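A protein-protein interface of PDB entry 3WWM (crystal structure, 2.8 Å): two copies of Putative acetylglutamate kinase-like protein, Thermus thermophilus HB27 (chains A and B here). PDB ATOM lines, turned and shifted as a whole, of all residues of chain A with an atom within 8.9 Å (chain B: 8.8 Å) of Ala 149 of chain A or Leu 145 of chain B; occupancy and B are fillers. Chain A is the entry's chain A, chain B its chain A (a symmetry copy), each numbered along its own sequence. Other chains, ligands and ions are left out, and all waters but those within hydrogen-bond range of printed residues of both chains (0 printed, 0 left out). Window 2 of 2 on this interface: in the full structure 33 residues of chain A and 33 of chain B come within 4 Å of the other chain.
Leu 142 of chain A touches Tyr 151 of chain B.
Ala 149 of chain B touches Leu 145 of chain A.
CB of Ala 149 of chain A touches CD2 of Leu 145 of chain B (3.95 Å).
OH of Tyr 151 of chain A touches CB of Leu 142 of chain B, 3.6 Å away.
The side-chain amide oxygen (OD1) of Asn 139 of chain B lies within hydrogen-bond range of the backbone NH (N) of Leu 142 of chain B (3.2 Å).
The side-chain amide oxygen (OD1) of Asn 139 of chain B sits close to the backbone NH (N) of Ala 141 of chain B (3.5 Å).
N of Tyr 151 of chain B lies within hydrogen-bond range of O of Leu 146 of chain B (3.0 Å).
O of Leu 146 of chain A lies within hydrogen-bond range of N of Tyr 151 of chain A (3.0 Å).
Leu 142 of chain A touches Tyr 151 of chain B, and with the chains exchanged Tyr 151 of chain A touches Leu 142 of chain B.
Leu 145 of chain A touches Ala 149 of chain B, and with the chains exchanged Ala 149 of chain A touches Leu 145 of chain B.
12 positions are printed for both chains.
Of the 5 pairs that touch across the chains among the printed residues, 4 have their exchanged pair printed and touching as well.
OH of Tyr 151 of chain A is in hydrogen-bond range of ND2 of Asn 139 of chain B (3.0 Å).
Of chain A, only Ala 149 comes within 4 Å of Leu 145 of chain B.
Gly 150 of chain A touches none of the printed residues of chain B.
Of the printed residues of chain A, Leu 142 of chain B touches Tyr 151 (3.6 Å).
Of the printed residues of chain B, Leu 142 of chain A touches Tyr 151.
Printed residues of chain B within 4 Å of Tyr 151 of chain A: Asn 139 (3.0 Å) and Leu 142 (3.6 Å).
Printed residues of chain A within 4 Å of Ala 149 of chain B: Leu 145 (3.95 Å).
Printed residues of chain B within 4 Å of Leu 145 of chain A: Ala 149.
The nearest residue of chain B that does not touch Ala 149 of chain A is Leu 142 of chain B (6.4 Å).
The nearest residue of chain A that does not touch Leu 145 of chain B is Leu 145 of chain A (4.3 Å).
The nearest printed residue of chain A that does not touch Ala 149 of chain B is Leu 142 of chain A (6.4 Å).
Along chain B the printed residues that touch a printed residue of chain A span positions 139 to 151.
Of the 16 printed residues of chain A, 4 touch a printed residue of chain B.
Printed residues of chain A that touch a printed residue of chain B: Leu 142, Leu 145, Ala 149 and Tyr 151.
Hydrophobic or aromatic side chains of chain A that line the printed part of chain B: Leu 142, Leu 145, Ala 149 and Tyr 151.
Among the printed residues, 5 pairs touch across the chains.
Among the printed residues, no Asp or Glu carboxylate lies within 4 Å of a Lys or Arg side-chain nitrogen of the other chain.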
ATOM      1  N   TRP A  25     -19.134   3.099   2.901  1.00  0.00           N
ATOM      2  CA  TRP A  25     -18.046   4.063   2.808  1.00  0.00           C
ATOM      3  C   TRP A  25     -16.761   3.360   2.362  1.00  0.00           C
ATOM      4  O   TRP A  25     -16.097   3.808   1.428  1.00  0.00           O
ATOM      5  CB  TRP A  25     -17.877   4.749   4.165  1.00  0.00           C
ATOM      6  CG  TRP A  25     -16.801   5.783   4.267  1.00  0.00           C
ATOM      7  CD1 TRP A  25     -16.891   7.102   3.934  1.00  0.00           C
ATOM      8  CD2 TRP A  25     -15.484   5.591   4.801  1.00  0.00           C
ATOM      9  NE1 TRP A  25     -15.699   7.742   4.212  1.00  0.00           N
ATOM     10  CE2 TRP A  25     -14.822   6.835   4.744  1.00  0.00           C
ATOM     11  CE3 TRP A  25     -14.794   4.481   5.305  1.00  0.00           C
ATOM     12  CZ2 TRP A  25     -13.507   6.999   5.174  1.00  0.00           C
ATOM     13  CZ3 TRP A  25     -13.485   4.646   5.734  1.00  0.00           C
ATOM     14  CH2 TRP A  25     -12.855   5.894   5.663  1.00  0.00           C
ATOM     15  N   LYS A  30     -20.025   7.556  -1.553  1.00  0.00           N
ATOM     16  CA  LYS A  30     -20.122   8.851  -0.885  1.00  0.00           C
ATOM     17  C   LYS A  30     -21.372   8.876  -0.009  1.00  0.00           C
ATOM     18  O   LYS A  30     -22.485   8.693  -0.503  1.00  0.00           O
ATOM     19  CB  LYS A  30     -20.196   9.988  -1.904  1.00  0.00           C
ATOM     20  CG  LYS A  30     -18.854  10.407  -2.487  1.00  0.00           C
ATOM     21  CD  LYS A  30     -18.273  11.607  -1.752  1.00  0.00           C
ATOM     22  CE  LYS A  30     -16.859  11.933  -2.225  1.00  0.00           C
ATOM     23  NZ  LYS A  30     -15.831  11.019  -1.644  1.00  0.00           N
ATOM     24  N   ASN A  96     -13.905   6.652   9.038  1.00  0.00           N
ATOM     25  CA  ASN A  96     -13.467   7.867   9.706  1.00  0.00           C
ATOM     26  C   ASN A  96     -14.577   8.914   9.698  1.00  0.00           C
ATOM     27  O   ASN A  96     -14.595   9.812   8.855  1.00  0.00           O
ATOM     28  CB  ASN A  96     -12.181   8.419   9.078  1.00  0.00           C
ATOM     29  CG  ASN A  96     -11.430   9.345  10.023  1.00  0.00           C
ATOM     30  OD1 ASN A  96     -11.950   9.746  11.059  1.00  0.00           O
ATOM     31  ND2 ASN A  96     -10.201   9.672   9.678  1.00  0.00           N
ATOM     32  N   ILE A  98     -16.955  12.034  11.056  1.00  0.00           N
ATOM     33  CA  ILE A  98     -16.782  13.324  11.688  1.00  0.00           C
ATOM     34  C   ILE A  98     -18.176  13.868  11.992  1.00  0.00           C
ATOM     35  O   ILE A  98     -19.020  13.991  11.105  1.00  0.00           O
ATOM     36  CB  ILE A  98     -15.934  14.267  10.809  1.00  0.00           C
ATOM     37  CG1 ILE A  98     -15.467  15.477  11.592  1.00  0.00           C
ATOM     38  CG2 ILE A  98     -16.693  14.735   9.577  1.00  0.00           C
ATOM     39  CD1 ILE A  98     -14.451  16.281  10.817  1.00  0.00           C
ATOM     40  N   ALA A 141     -19.297  24.217   1.116  1.00  0.00           N
ATOM     41  CA  ALA A 141     -17.841  24.280   0.999  1.00  0.00           C
ATOM     42  C   ALA A 141     -17.180  23.400   2.054  1.00  0.00           C
ATOM     43  O   ALA A 141     -16.264  22.626   1.752  1.00  0.00           O
ATOM     44  CB  ALA A 141     -17.362  25.710   1.142  1.00  0.00           C
ATOM     45  N   LEU A 142     -17.665  23.515   3.290  1.00  0.00           N
ATOM     46  CA  LEU A 142     -17.130  22.745   4.407  1.00  0.00           C
ATOM     47  C   LEU A 142     -17.365  21.258   4.203  1.00  0.00           C
ATOM     48  O   LEU A 142     -16.444  20.457   4.345  1.00  0.00           O
ATOM     49  CB  LEU A 142     -17.766  23.202   5.715  1.00  0.00           C
ATOM     50  CG  LEU A 142     -17.394  22.400   6.959  1.00  0.00           C
ATOM     51  CD1 LEU A 142     -15.898  22.468   7.224  1.00  0.00           C
ATOM     52  CD2 LEU A 142     -18.191  22.915   8.149  1.00  0.00           C
ATOM     53  N   LEU A 143     -18.595  20.888   3.863  1.00  0.00           N
ATOM     54  CA  LEU A 143     -18.910  19.489   3.591  1.00  0.00           C
ATOM     55  C   LEU A 143     -18.060  18.938   2.449  1.00  0.00           C
ATOM     56  O   LEU A 143     -17.512  17.843   2.560  1.00  0.00           O
ATOM     57  CB  LEU A 143     -20.391  19.310   3.275  1.00  0.00           C
ATOM     58  CG  LEU A 143     -21.340  19.496   4.457  1.00  0.00           C
ATOM     59  CD1 LEU A 143     -22.778  19.281   4.012  1.00  0.00           C
ATOM     60  CD2 LEU A 143     -21.003  18.557   5.602  1.00  0.00           C
ATOM     61  N   ASP A 144     -17.950  19.699   1.363  1.00  0.00           N
ATOM     62  CA  ASP A 144     -17.109  19.314   0.233  1.00  0.00           C
ATOM     63  C   ASP A 144     -15.675  19.103   0.691  1.00  0.00           C
ATOM     64  O   ASP A 144     -15.022  18.136   0.306  1.00  0.00           O
ATOM     65  CB  ASP A 144     -17.121  20.394  -0.856  1.00  0.00           C
ATOM     66  CG  ASP A 144     -18.423  20.440  -1.637  1.00  0.00           C
ATOM     67  OD1 ASP A 144     -19.231  19.491  -1.546  1.00  0.00           O
ATOM     68  OD2 ASP A 144     -18.630  21.442  -2.357  1.00  0.00           O
ATOM     69  N   LEU A 145     -15.195  20.025   1.516  1.00  0.00           N
ATOM     70  CA  LEU A 145     -13.820  19.992   1.990  1.00  0.00           C
ATOM     71  C   LEU A 145     -13.550  18.724   2.787  1.00  0.00           C
ATOM     72  O   LEU A 145     -12.539  18.059   2.573  1.00  0.00           O
ATOM     73  CB  LEU A 145     -13.557  21.211   2.866  1.00  0.00           C
ATOM     74  CG  LEU A 145     -12.125  21.457   3.306  1.00  0.00           C
ATOM     75  CD1 LEU A 145     -11.309  21.921   2.118  1.00  0.00           C
ATOM     76  CD2 LEU A 145     -12.117  22.493   4.420  1.00  0.00           C
ATOM     77  N   LEU A 146     -14.455  18.403   3.710  1.00  0.00           N
ATOM     78  CA  LEU A 146     -14.317  17.214   4.534  1.00  0.00           C
ATOM     79  C   LEU A 146     -14.481  15.933   3.711  1.00  0.00           C
ATOM     80  O   LEU A 146     -13.771  14.947   3.953  1.00  0.00           O
ATOM     81  CB  LEU A 146     -15.322  17.245   5.683  1.00  0.00           C
ATOM     82  CG  LEU A 146     -15.151  18.370   6.708  1.00  0.00           C
ATOM     83  CD1 LEU A 146     -16.273  18.315   7.729  1.00  0.00           C
ATOM     84  CD2 LEU A 146     -13.805  18.291   7.411  1.00  0.00           C
ATOM     85  N   LEU A 147     -15.402  15.949   2.745  1.00  0.00           N
ATOM     86  CA  LEU A 147     -15.606  14.803   1.850  1.00  0.00           C
ATOM     87  C   LEU A 147     -14.367  14.539   0.985  1.00  0.00           C
ATOM     88  O   LEU A 147     -13.943  13.398   0.843  1.00  0.00           O
ATOM     89  CB  LEU A 147     -16.829  15.008   0.948  1.00  0.00           C
ATOM     90  CG  LEU A 147     -18.224  14.939   1.588  1.00  0.00           C
ATOM     91  CD1 LEU A 147     -19.256  15.548   0.649  1.00  0.00           C
ATOM     92  CD2 LEU A 147     -18.629  13.521   1.969  1.00  0.00           C
ATOM     93  N   GLN A 148     -13.787  15.597   0.424  1.00  0.00           N
ATOM     94  CA  GLN A 148     -12.571  15.483  -0.380  1.00  0.00           C
ATOM     95  C   GLN A 148     -11.394  14.917   0.406  1.00  0.00           C
ATOM     96  O   GLN A 148     -10.579  14.176  -0.138  1.00  0.00           O
ATOM     97  CB  GLN A 148     -12.194  16.841  -0.966  1.00  0.00           C
ATOM     98  CG  GLN A 148     -13.124  17.276  -2.095  1.00  0.00           C
ATOM     99  CD  GLN A 148     -12.885  18.707  -2.548  1.00  0.00           C
ATOM    100  OE1 GLN A 148     -11.853  19.311  -2.225  1.00  0.00           O
ATOM    101  NE2 GLN A 148     -13.836  19.256  -3.307  1.00  0.00           N
ATOM    102  N   ALA A 149     -11.314  15.271   1.685  1.00  0.00           N
ATOM    103  CA  ALA A 149     -10.270  14.771   2.566  1.00  0.00           C
ATOM    104  C   ALA A 149     -10.555  13.349   3.039  1.00  0.00           C
ATOM    105  O   ALA A 149      -9.719  12.746   3.705  1.00  0.00           O
ATOM    106  CB  ALA A 149     -10.108  15.698   3.759  1.00  0.00           C
ATOM    107  N   GLY A 150     -11.746  12.834   2.732  1.00  0.00           N
ATOM    108  CA  GLY A 150     -12.081  11.433   2.978  1.00  0.00           C
ATOM    109  C   GLY A 150     -12.878  11.123   4.242  1.00  0.00           C
ATOM    110  O   GLY A 150     -13.151   9.955   4.517  1.00  0.00           O
ATOM    111  N   TYR A 151     -13.272  12.144   5.004  1.00  0.00           N
ATOM    112  CA  TYR A 151     -14.064  11.925   6.217  1.00  0.00           C
ATOM    113  C   TYR A 151     -15.515  11.620   5.850  1.00  0.00           C
ATOM    114  O   TYR A 151     -15.966  11.958   4.754  1.00  0.00           O
ATOM    115  CB  TYR A 151     -13.967  13.131   7.153  1.00  0.00           C
ATOM    116  CG  TYR A 151     -12.540  13.429   7.559  1.00  0.00           C
ATOM    117  CD1 TYR A 151     -11.935  12.748   8.615  1.00  0.00           C
ATOM    118  CD2 TYR A 151     -11.784  14.364   6.867  1.00  0.00           C
ATOM    119  CE1 TYR A 151     -10.622  13.005   8.979  1.00  0.00           C
ATOM    120  CE2 TYR A 151     -10.470  14.627   7.222  1.00  0.00           C
ATOM    121  CZ  TYR A 151      -9.894  13.945   8.277  1.00  0.00           C
ATOM    122  OH  TYR A 151      -8.587  14.205   8.615  1.00  0.00           O
ATOM    123  N   LEU A 152     -16.223  10.945   6.755  1.00  0.00           N
ATOM    124  CA  LEU A 152     -17.644  10.623   6.574  1.00  0.00           C
ATOM    125  C   LEU A 152     -18.476  11.491   7.525  1.00  0.00           C
ATOM    126  O   LEU A 152     -18.551  11.201   8.713  1.00  0.00           O
ATOM    127  CB  LEU A 152     -17.888   9.133   6.822  1.00  0.00           C
ATOM    128  CG  LEU A 152     -19.306   8.595   7.044  1.00  0.00           C
ATOM    129  CD1 LEU A 152     -20.350   9.235   6.150  1.00  0.00           C
ATOM    130  CD2 LEU A 152     -19.314   7.097   6.831  1.00  0.00           C
ATOM    131  N   ILE B  98     -15.769  26.032  14.985  1.00  0.00           N
ATOM    132  CA  ILE B  98     -16.147  24.678  14.645  1.00  0.00           C
ATOM    133  C   ILE B  98     -15.811  23.800  15.849  1.00  0.00           C
ATOM    134  O   ILE B  98     -14.673  23.771  16.318  1.00  0.00           O
ATOM    135  CB  ILE B  98     -15.463  24.218  13.341  1.00  0.00           C
ATOM    136  CG1 ILE B  98     -16.101  22.954  12.802  1.00  0.00           C
ATOM    137  CG2 ILE B  98     -13.973  23.980  13.531  1.00  0.00           C
ATOM    138  CD1 ILE B  98     -15.600  22.629  11.415  1.00  0.00           C
ATOM    139  N   ASN B 139      -4.801  14.355  15.194  1.00  0.00           N
ATOM    140  CA  ASN B 139      -4.977  14.439  13.752  1.00  0.00           C
ATOM    141  C   ASN B 139      -4.697  15.874  13.347  1.00  0.00           C
ATOM    142  O   ASN B 139      -5.611  16.660  13.091  1.00  0.00           O
ATOM    143  CB  ASN B 139      -6.377  13.990  13.328  1.00  0.00           C
ATOM    144  CG  ASN B 139      -6.564  14.002  11.825  1.00  0.00           C
ATOM    145  OD1 ASN B 139      -5.688  14.424  11.076  1.00  0.00           O
ATOM    146  ND2 ASN B 139      -7.724  13.550  11.378  1.00  0.00           N
ATOM    147  N   LYS B 140      -3.415  16.214  13.306  1.00  0.00           N
ATOM    148  CA  LYS B 140      -3.009  17.570  13.011  1.00  0.00           C
ATOM    149  C   LYS B 140      -3.383  17.971  11.576  1.00  0.00           C
ATOM    150  O   LYS B 140      -3.645  19.143  11.311  1.00  0.00           O
ATOM    151  CB  LYS B 140      -1.513  17.738  13.256  1.00  0.00           C
ATOM    152  CG  LYS B 140      -1.060  19.187  13.286  1.00  0.00           C
ATOM    153  CD  LYS B 140       0.397  19.291  13.683  1.00  0.00           C
ATOM    154  CE  LYS B 140       0.890  20.726  13.610  1.00  0.00           C
ATOM    155  NZ  LYS B 140       0.834  21.266  12.226  1.00  0.00           N
ATOM    156  N   ALA B 141      -3.419  17.005  10.662  1.00  0.00           N
ATOM    157  CA  ALA B 141      -3.826  17.272   9.282  1.00  0.00           C
ATOM    158  C   ALA B 141      -5.202  17.927   9.247  1.00  0.00           C
ATOM    159  O   ALA B 141      -5.414  18.924   8.545  1.00  0.00           O
ATOM    160  CB  ALA B 141      -3.841  15.990   8.478  1.00  0.00           C
ATOM    161  N   LEU B 142      -6.130  17.367  10.024  1.00  0.00           N
ATOM    162  CA  LEU B 142      -7.495  17.875  10.090  1.00  0.00           C
ATOM    163  C   LEU B 142      -7.524  19.279  10.670  1.00  0.00           C
ATOM    164  O   LEU B 142      -8.146  20.175  10.105  1.00  0.00           O
ATOM    165  CB  LEU B 142      -8.364  16.944  10.928  1.00  0.00           C
ATOM    166  CG  LEU B 142      -9.792  17.414  11.189  1.00  0.00           C
ATOM    167  CD1 LEU B 142     -10.560  17.575   9.886  1.00  0.00           C
ATOM    168  CD2 LEU B 142     -10.484  16.428  12.121  1.00  0.00           C
ATOM    169  N   LEU B 143      -6.844  19.475  11.796  1.00  0.00           N
ATOM    170  CA  LEU B 143      -6.764  20.800  12.403  1.00  0.00           C
ATOM    171  C   LEU B 143      -6.143  21.816  11.447  1.00  0.00           C
ATOM    172  O   LEU B 143      -6.662  22.920  11.296  1.00  0.00           O
ATOM    173  CB  LEU B 143      -5.978  20.761  13.709  1.00  0.00           C
ATOM    174  CG  LEU B 143      -6.675  20.056  14.871  1.00  0.00           C
ATOM    175  CD1 LEU B 143      -5.793  20.094  16.110  1.00  0.00           C
ATOM    176  CD2 LEU B 143      -8.027  20.674  15.174  1.00  0.00           C
ATOM    177  N   ASP B 144      -5.041  21.437  10.805  1.00  0.00           N
ATOM    178  CA  ASP B 144      -4.393  22.292   9.814  1.00  0.00           C
ATOM    179  C   ASP B 144      -5.370  22.647   8.705  1.00  0.00           C
ATOM    180  O   ASP B 144      -5.450  23.794   8.273  1.00  0.00           O
ATOM    181  CB  ASP B 144      -3.179  21.590   9.191  1.00  0.00           C
ATOM    182  CG  ASP B 144      -1.989  21.508  10.129  1.00  0.00           C
ATOM    183  OD1 ASP B 144      -1.971  22.209  11.165  1.00  0.00           O
ATOM    184  OD2 ASP B 144      -1.057  20.736   9.817  1.00  0.00           O
ATOM    185  N   LEU B 145      -6.109  21.643   8.249  1.00  0.00           N
ATOM    186  CA  LEU B 145      -7.044  21.814   7.148  1.00  0.00           C
ATOM    187  C   LEU B 145      -8.122  22.828   7.503  1.00  0.00           C
ATOM    188  O   LEU B 145      -8.427  23.716   6.710  1.00  0.00           O
ATOM    189  CB  LEU B 145      -7.691  20.474   6.819  1.00  0.00           C
ATOM    190  CG  LEU B 145      -8.559  20.406   5.576  1.00  0.00           C
ATOM    191  CD1 LEU B 145      -7.678  20.477   4.346  1.00  0.00           C
ATOM    192  CD2 LEU B 145      -9.368  19.117   5.602  1.00  0.00           C
ATOM    193  N   LEU B 146      -8.700  22.681   8.694  1.00  0.00           N
ATOM    194  CA  LEU B 146      -9.740  23.585   9.155  1.00  0.00           C
ATOM    195  C   LEU B 146      -9.190  24.989   9.427  1.00  0.00           C
ATOM    196  O   LEU B 146      -9.865  25.985   9.136  1.00  0.00           O
ATOM    197  CB  LEU B 146     -10.418  23.023  10.402  1.00  0.00           C
ATOM    198  CG  LEU B 146     -11.186  21.710  10.229  1.00  0.00           C
ATOM    199  CD1 LEU B 146     -11.722  21.243  11.570  1.00  0.00           C
ATOM    200  CD2 LEU B 146     -12.327  21.854   9.236  1.00  0.00           C
ATOM    201  N   LEU B 147      -7.975  25.064   9.973  1.00  0.00           N
ATOM    202  CA  LEU B 147      -7.317  26.354  10.221  1.00  0.00           C
ATOM    203  C   LEU B 147      -7.030  27.099   8.912  1.00  0.00           C
ATOM    204  O   LEU B 147      -7.284  28.293   8.811  1.00  0.00           O
ATOM    205  CB  LEU B 147      -6.012  26.175  11.008  1.00  0.00           C
ATOM    206  CG  LEU B 147      -6.106  25.775  12.488  1.00  0.00           C
ATOM    207  CD1 LEU B 147      -4.755  25.266  12.974  1.00  0.00           C
ATOM    208  CD2 LEU B 147      -6.591  26.912  13.378  1.00  0.00           C
ATOM    209  N   GLN B 148      -6.515  26.386   7.913  1.00  0.00           N
ATOM    210  CA  GLN B 148      -6.245  26.970   6.599  1.00  0.00           C
ATOM    211  C   GLN B 148      -7.500  27.511   5.924  1.00  0.00           C
ATOM    212  O   GLN B 148      -7.449  28.524   5.232  1.00  0.00           O
ATOM    213  CB  GLN B 148      -5.574  25.941   5.692  1.00  0.00           C
ATOM    214  CG  GLN B 148      -4.124  25.671   6.077  1.00  0.00           C
ATOM    215  CD  GLN B 148      -3.508  24.509   5.314  1.00  0.00           C
ATOM    216  OE1 GLN B 148      -4.054  24.059   4.298  1.00  0.00           O
ATOM    217  NE2 GLN B 148      -2.363  24.021   5.797  1.00  0.00           N
ATOM    218  N   ALA B 149      -8.623  26.828   6.130  1.00  0.00           N
ATOM    219  CA  ALA B 149      -9.902  27.253   5.585  1.00  0.00           C
ATOM    220  C   ALA B 149     -10.516  28.392   6.394  1.00  0.00           C
ATOM    221  O   ALA B 149     -11.546  28.933   6.004  1.00  0.00           O
ATOM    222  CB  ALA B 149     -10.861  26.076   5.527  1.00  0.00           C
ATOM    223  N   GLY B 150      -9.910  28.722   7.535  1.00  0.00           N
ATOM    224  CA  GLY B 150     -10.296  29.896   8.315  1.00  0.00           C
ATOM    225  C   GLY B 150     -11.222  29.663   9.506  1.00  0.00           C
ATOM    226  O   GLY B 150     -11.608  30.623  10.172  1.00  0.00           O
ATOM    227  N   TYR B 151     -11.567  28.409   9.799  1.00  0.00           N
ATOM    228  CA  TYR B 151     -12.429  28.107  10.943  1.00  0.00           C
ATOM    229  C   TYR B 151     -11.633  28.205  12.243  1.00  0.00           C
ATOM    230  O   TYR B 151     -10.404  28.113  12.231  1.00  0.00           O
ATOM    231  CB  TYR B 151     -13.074  26.728  10.787  1.00  0.00           C
ATOM    232  CG  TYR B 151     -13.898  26.620   9.524  1.00  0.00           C
ATOM    233  CD1 TYR B 151     -15.216  27.076   9.483  1.00  0.00           C
ATOM    234  CD2 TYR B 151     -13.353  26.095   8.361  1.00  0.00           C
ATOM    235  CE1 TYR B 151     -15.970  26.995   8.321  1.00  0.00           C
ATOM    236  CE2 TYR B 151     -14.098  26.012   7.195  1.00  0.00           C
ATOM    237  CZ  TYR B 151     -15.404  26.464   7.180  1.00  0.00           C
ATOM    238  OH  TYR B 151     -16.132  26.386   6.016  1.00  0.00           O
ATOM    239  N   PRO B 153     -11.194  26.264  15.577  1.00  0.00           N
ATOM    240  CA  PRO B 153     -11.531  24.989  16.209  1.00  0.00           C
ATOM    241  C   PRO B 153     -11.746  25.099  17.716  1.00  0.00           C
ATOM    242  O   PRO B 153     -10.937  25.708  18.417  1.00  0.00           O
ATOM    243  CB  PRO B 153     -10.307  24.113  15.908  1.00  0.00           C
ATOM    244  CG  PRO B 153      -9.614  24.787  14.771  1.00  0.00           C
ATOM    245  CD  PRO B 153      -9.819  26.241  15.048  1.00  0.00           C
ATOM    246  N   TYR B 182       2.260  22.475  17.604  1.00  0.00           N
ATOM    247  CA  TYR B 182       2.194  23.689  16.797  1.00  0.00           C
ATOM    248  C   TYR B 182       3.302  24.713  17.085  1.00  0.00           C
ATOM    249  O   TYR B 182       3.372  25.744  16.416  1.00  0.00           O
ATOM    250  CB  TYR B 182       0.826  24.349  16.958  1.00  0.00           C
ATOM    251  CG  TYR B 182      -0.230  23.719  16.082  1.00  0.00           C
ATOM    252  CD1 TYR B 182      -0.979  22.631  16.526  1.00  0.00           C
ATOM    253  CD2 TYR B 182      -0.468  24.202  14.798  1.00  0.00           C
ATOM    254  CE1 TYR B 182      -1.942  22.048  15.718  1.00  0.00           C
ATOM    255  CE2 TYR B 182      -1.423  23.626  13.986  1.00  0.00           C
ATOM    256  CZ  TYR B 182      -2.159  22.551  14.444  1.00  0.00           C
ATOM    257  OH  TYR B 182      -3.113  21.980  13.626  1.00  0.00           O
